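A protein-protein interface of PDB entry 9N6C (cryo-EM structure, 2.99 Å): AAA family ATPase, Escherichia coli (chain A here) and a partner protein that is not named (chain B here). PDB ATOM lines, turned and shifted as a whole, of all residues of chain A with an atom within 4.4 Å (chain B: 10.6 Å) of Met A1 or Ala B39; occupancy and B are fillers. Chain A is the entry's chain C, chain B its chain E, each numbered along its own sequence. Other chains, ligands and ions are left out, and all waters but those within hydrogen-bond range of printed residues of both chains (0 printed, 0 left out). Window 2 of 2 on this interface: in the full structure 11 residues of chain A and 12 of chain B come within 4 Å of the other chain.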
ATOM      1  N   MET A   1      -4.724  29.287  -1.573  1.00  0.00           N
ATOM      2  CA  MET A   1      -3.937  28.261  -0.901  1.00  0.00           C
ATOM      3  C   MET A   1      -4.252  26.875  -1.452  1.00  0.00           C
ATOM      4  O   MET A   1      -4.250  25.894  -0.714  1.00  0.00           O
ATOM      5  CB  MET A   1      -4.185  28.299   0.607  1.00  0.00           C
ATOM      6  CG  MET A   1      -4.455  29.690   1.146  1.00  0.00           C
ATOM      7  SD  MET A   1      -6.180  30.167   0.962  1.00  0.00           S
ATOM      8  CE  MET A   1      -6.900  29.359   2.385  1.00  0.00           C
ATOM      9  N   TRP A   2      -4.526  26.800  -2.751  1.00  0.00           N
ATOM     10  CA  TRP A   2      -4.872  25.541  -3.387  1.00  0.00           C
ATOM     11  C   TRP A   2      -4.518  25.623  -4.866  1.00  0.00           C
ATOM     12  O   TRP A   2      -4.068  26.660  -5.362  1.00  0.00           O
ATOM     13  CB  TRP A   2      -6.352  25.213  -3.177  1.00  0.00           C
ATOM     14  N   HIS A   4      -5.741  24.967  -8.955  1.00  0.00           N
ATOM     15  CA  HIS A   4      -6.910  25.092  -9.808  1.00  0.00           C
ATOM     16  C   HIS A   4      -6.549  24.720 -11.237  1.00  0.00           C
ATOM     17  O   HIS A   4      -5.366  24.655 -11.591  1.00  0.00           O
ATOM     18  CB  HIS A   4      -7.470  26.522  -9.767  1.00  0.00           C
ATOM     19  CG  HIS A   4      -8.074  26.894  -8.452  1.00  0.00           C
ATOM     20  ND1 HIS A   4      -8.350  28.197  -8.103  1.00  0.00           N
ATOM     21  CD2 HIS A   4      -8.466  26.133  -7.404  1.00  0.00           C
ATOM     22  CE1 HIS A   4      -8.881  28.223  -6.894  1.00  0.00           C
ATOM     23  NE2 HIS A   4      -8.961  26.984  -6.447  1.00  0.00           N
ATOM     24  N   GLU A  16      -1.684  37.483  -7.597  1.00  0.00           N
ATOM     25  CA  GLU A  16      -2.429  36.263  -7.306  1.00  0.00           C
ATOM     26  C   GLU A  16      -2.327  35.269  -8.456  1.00  0.00           C
ATOM     27  O   GLU A  16      -2.178  34.058  -8.235  1.00  0.00           O
ATOM     28  CB  GLU A  16      -3.888  36.605  -7.015  1.00  0.00           C
ATOM     29  CG  GLU A  16      -4.791  35.401  -6.849  1.00  0.00           C
ATOM     30  CD  GLU A  16      -5.992  35.702  -5.978  1.00  0.00           C
ATOM     31  OE1 GLU A  16      -6.742  36.646  -6.303  1.00  0.00           O
ATOM     32  OE2 GLU A  16      -6.186  34.999  -4.965  1.00  0.00           O
ATOM     33  N   TYR A  19       0.930  33.599  -8.435  1.00  0.00           N
ATOM     34  CA  TYR A  19       0.973  32.665  -7.321  1.00  0.00           C
ATOM     35  C   TYR A  19       0.295  31.361  -7.695  1.00  0.00           C
ATOM     36  O   TYR A  19       0.773  30.280  -7.336  1.00  0.00           O
ATOM     37  CB  TYR A  19       0.310  33.285  -6.093  1.00  0.00           C
ATOM     38  CG  TYR A  19       0.114  32.327  -4.942  1.00  0.00           C
ATOM     39  CD1 TYR A  19       1.174  31.591  -4.438  1.00  0.00           C
ATOM     40  CD2 TYR A  19      -1.134  32.160  -4.360  1.00  0.00           C
ATOM     41  CE1 TYR A  19       0.997  30.717  -3.387  1.00  0.00           C
ATOM     42  CE2 TYR A  19      -1.319  31.288  -3.310  1.00  0.00           C
ATOM     43  CZ  TYR A  19      -0.250  30.570  -2.827  1.00  0.00           C
ATOM     44  OH  TYR A  19      -0.428  29.699  -1.780  1.00  0.00           O
ATOM     45  N   LEU A 163      -9.951  34.688   5.577  1.00  0.00           N
ATOM     46  CA  LEU A 163      -9.455  34.117   4.325  1.00  0.00           C
ATOM     47  C   LEU A 163      -8.343  34.958   3.698  1.00  0.00           C
ATOM     48  O   LEU A 163      -7.334  34.412   3.225  1.00  0.00           O
ATOM     49  CB  LEU A 163     -10.611  33.956   3.341  1.00  0.00           C
ATOM     50  CG  LEU A 163     -10.524  32.815   2.328  1.00  0.00           C
ATOM     51  CD1 LEU A 163      -9.720  31.654   2.886  1.00  0.00           C
ATOM     52  CD2 LEU A 163     -11.915  32.358   1.926  1.00  0.00           C
ATOM     53  N   LYS A 167      -4.404  33.818   2.992  1.00  0.00           N
ATOM     54  CA  LYS A 167      -3.919  33.734   1.625  1.00  0.00           C
ATOM     55  C   LYS A 167      -2.638  34.538   1.487  1.00  0.00           C
ATOM     56  O   LYS A 167      -1.689  34.101   0.828  1.00  0.00           O
ATOM     57  CB  LYS A 167      -4.983  34.229   0.648  1.00  0.00           C
ATOM     58  CG  LYS A 167      -4.605  34.049  -0.810  1.00  0.00           C
ATOM     59  CD  LYS A 167      -5.474  34.898  -1.718  1.00  0.00           C
ATOM     60  CE  LYS A 167      -6.945  34.668  -1.443  1.00  0.00           C
ATOM     61  NZ  LYS A 167      -7.792  35.711  -2.081  1.00  0.00           N
ATOM     62  N   SER A 170       0.360  32.779   3.070  1.00  0.00           N
ATOM     63  CA  SER A 170       0.859  31.620   2.344  1.00  0.00           C
ATOM     64  C   SER A 170       1.872  32.022   1.281  1.00  0.00           C
ATOM     65  O   SER A 170       2.818  31.271   1.019  1.00  0.00           O
ATOM     66  CB  SER A 170      -0.300  30.859   1.708  1.00  0.00           C
ATOM     67  OG  SER A 170      -1.357  30.684   2.633  1.00  0.00           O
ATOM     68  N   ILE B  34     -16.195  23.169  -4.465  1.00  0.00           N
ATOM     69  CA  ILE B  34     -16.114  23.685  -5.831  1.00  0.00           C
ATOM     70  C   ILE B  34     -14.964  24.680  -5.923  1.00  0.00           C
ATOM     71  O   ILE B  34     -14.687  25.399  -4.951  1.00  0.00           O
ATOM     72  CB  ILE B  34     -17.435  24.324  -6.291  1.00  0.00           C
ATOM     73  CG1 ILE B  34     -17.886  25.404  -5.319  1.00  0.00           C
ATOM     74  CG2 ILE B  34     -18.509  23.268  -6.454  1.00  0.00           C
ATOM     75  CD1 ILE B  34     -18.982  26.277  -5.869  1.00  0.00           C
ATOM     76  N   PRO B  35     -14.275  24.757  -7.060  1.00  0.00           N
ATOM     77  CA  PRO B  35     -13.151  25.688  -7.182  1.00  0.00           C
ATOM     78  C   PRO B  35     -13.617  27.133  -7.175  1.00  0.00           C
ATOM     79  O   PRO B  35     -14.753  27.449  -7.531  1.00  0.00           O
ATOM     80  CB  PRO B  35     -12.525  25.314  -8.529  1.00  0.00           C
ATOM     81  CG  PRO B  35     -13.629  24.694  -9.292  1.00  0.00           C
ATOM     82  CD  PRO B  35     -14.473  23.972  -8.289  1.00  0.00           C
ATOM     83  N   LYS B  36     -12.714  28.010  -6.757  1.00  0.00           N
ATOM     84  CA  LYS B  36     -12.972  29.437  -6.679  1.00  0.00           C
ATOM     85  C   LYS B  36     -12.236  30.160  -7.799  1.00  0.00           C
ATOM     86  O   LYS B  36     -11.173  29.725  -8.246  1.00  0.00           O
ATOM     87  CB  LYS B  36     -12.537  29.992  -5.322  1.00  0.00           C
ATOM     88  CG  LYS B  36     -13.537  30.923  -4.676  1.00  0.00           C
ATOM     89  CD  LYS B  36     -13.211  31.133  -3.210  1.00  0.00           C
ATOM     90  CE  LYS B  36     -14.120  32.175  -2.593  1.00  0.00           C
ATOM     91  NZ  LYS B  36     -13.962  32.232  -1.118  1.00  0.00           N
ATOM     92  N   ARG B  37     -12.816  31.264  -8.255  1.00  0.00           N
ATOM     93  CA  ARG B  37     -12.182  32.102  -9.270  1.00  0.00           C
ATOM     94  C   ARG B  37     -11.037  32.859  -8.613  1.00  0.00           C
ATOM     95  O   ARG B  37     -11.234  33.914  -8.008  1.00  0.00           O
ATOM     96  CB  ARG B  37     -13.196  33.051  -9.893  1.00  0.00           C
ATOM     97  CG  ARG B  37     -14.163  32.369 -10.839  1.00  0.00           C
ATOM     98  CD  ARG B  37     -15.149  33.352 -11.434  1.00  0.00           C
ATOM     99  NE  ARG B  37     -16.347  32.685 -11.930  1.00  0.00           N
ATOM    100  CZ  ARG B  37     -17.490  33.300 -12.196  1.00  0.00           C
ATOM    101  NH1 ARG B  37     -17.628  34.604 -12.029  1.00  0.00           N
ATOM    102  NH2 ARG B  37     -18.520  32.589 -12.644  1.00  0.00           N
ATOM    103  N   GLY B  38      -9.829  32.315  -8.732  1.00  0.00           N
ATOM    104  CA  GLY B  38      -8.686  32.822  -8.002  1.00  0.00           C
ATOM    105  C   GLY B  38      -8.003  31.715  -7.226  1.00  0.00           C
ATOM    106  O   GLY B  38      -7.438  30.796  -7.826  1.00  0.00           O
ATOM    107  N   ALA B  39      -8.048  31.781  -5.899  1.00  0.00           N
ATOM    108  CA  ALA B  39      -7.489  30.727  -5.064  1.00  0.00           C
ATOM    109  C   ALA B  39      -8.436  30.466  -3.907  1.00  0.00           C
ATOM    110  O   ALA B  39      -8.904  31.407  -3.261  1.00  0.00           O
ATOM    111  CB  ALA B  39      -6.100  31.107  -4.542  1.00  0.00           C
ATOM    112  N   GLY B  40      -8.718  29.188  -3.652  1.00  0.00           N
ATOM    113  CA  GLY B  40      -9.565  28.776  -2.559  1.00  0.00           C
ATOM    114  C   GLY B  40     -10.577  27.757  -3.030  1.00  0.00           C
ATOM    115  O   GLY B  40     -10.433  27.157  -4.100  1.00  0.00           O
ATOM    116  N   PHE B  41     -11.612  27.560  -2.217  1.00  0.00           N
ATOM    117  CA  PHE B  41     -12.657  26.594  -2.512  1.00  0.00           C
ATOM    118  C   PHE B  41     -13.937  27.027  -1.814  1.00  0.00           C
ATOM    119  O   PHE B  41     -13.921  27.877  -0.921  1.00  0.00           O
ATOM    120  CB  PHE B  41     -12.264  25.183  -2.060  1.00  0.00           C
ATOM    121  CG  PHE B  41     -11.433  24.433  -3.058  1.00  0.00           C
ATOM    122  CD1 PHE B  41     -11.992  23.964  -4.230  1.00  0.00           C
ATOM    123  CD2 PHE B  41     -10.093  24.193  -2.821  1.00  0.00           C
ATOM    124  CE1 PHE B  41     -11.232  23.271  -5.148  1.00  0.00           C
ATOM    125  CE2 PHE B  41      -9.328  23.502  -3.737  1.00  0.00           C
ATOM    126  CZ  PHE B  41      -9.897  23.042  -4.901  1.00  0.00           C
ATOM    127  N   ARG B  42     -15.051  26.431  -2.230  1.00  0.00           N
ATOM    128  CA  ARG B  42     -16.350  26.746  -1.656  1.00  0.00           C
ATOM    129  C   ARG B  42     -17.053  25.447  -1.287  1.00  0.00           C
ATOM    130  O   ARG B  42     -16.798  24.395  -1.875  1.00  0.00           O
ATOM    131  CB  ARG B  42     -17.215  27.563  -2.619  1.00  0.00           C
ATOM    132  CG  ARG B  42     -18.168  28.522  -1.936  1.00  0.00           C
ATOM    133  CD  ARG B  42     -18.917  29.362  -2.951  1.00  0.00           C
ATOM    134  NE  ARG B  42     -18.368  30.706  -3.071  1.00  0.00           N
ATOM    135  CZ  ARG B  42     -18.696  31.718  -2.280  1.00  0.00           C
ATOM    136  NH1 ARG B  42     -19.565  31.573  -1.296  1.00  0.00           N
ATOM    137  NH2 ARG B  42     -18.141  32.908  -2.488  1.00  0.00           N
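Of the 9 printed residues of chain B, 5 touch a printed residue of chain A.
Hydrophobic or aromatic side chains of chain B within 4 Å of the printed part of chain A: Ala B39 and Phe B41.
Among the printed residues, 8 pairs touch across the chains.
A ring nitrogen (NE2) of His A4 is in hydrogen-bond range of the backbone carbonyl oxygen of Gly B40.
The backbone carbonyl oxygen of Lys B36 sits close to a ring nitrogen (ND1) of His A4 (3.2 Å).
O of Gly B38 sits at hydrogen-bond distance from ND1 of His A4 (2.8 Å).
Of the printed residues of chain B, Met A1 touches Ala B39 (3.7 Å).
Of chain B, only Phe B41 comes within 4 Å of Trp A2.
Of the printed residues of chain B, Leu A163 touches Lys B36.
No residue of chain B comes within 4 Å of Lys A167.
Printed residues of chain A within 4 Å of Lys B36: His A4 and Leu A163.
Arg B37 touches none of the printed residues of chain A.
Ala B39 touches just these residues of chain A: Met A1, His A4 and Glu A16.
Printed residues of chain A within 4 Å of Phe B41: Trp A2.
The side-chain carboxylate of Glu A16 lies within salt-bridge range of the side-chain amino group of Lys A167, 3.4 Å away.
Ala B39 touches Met A1.
CB of Trp A2 touches CE2 of Phe B41 (3.5 Å).
CE1 of His A4 touches CA of Ala B39, at 3.4 Å.
Ala B39 touches Glu A16 (N to OE2, 3.8 Å).
NZ of Lys B36 touches CD2 of Leu A163, at 3.7 Å.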
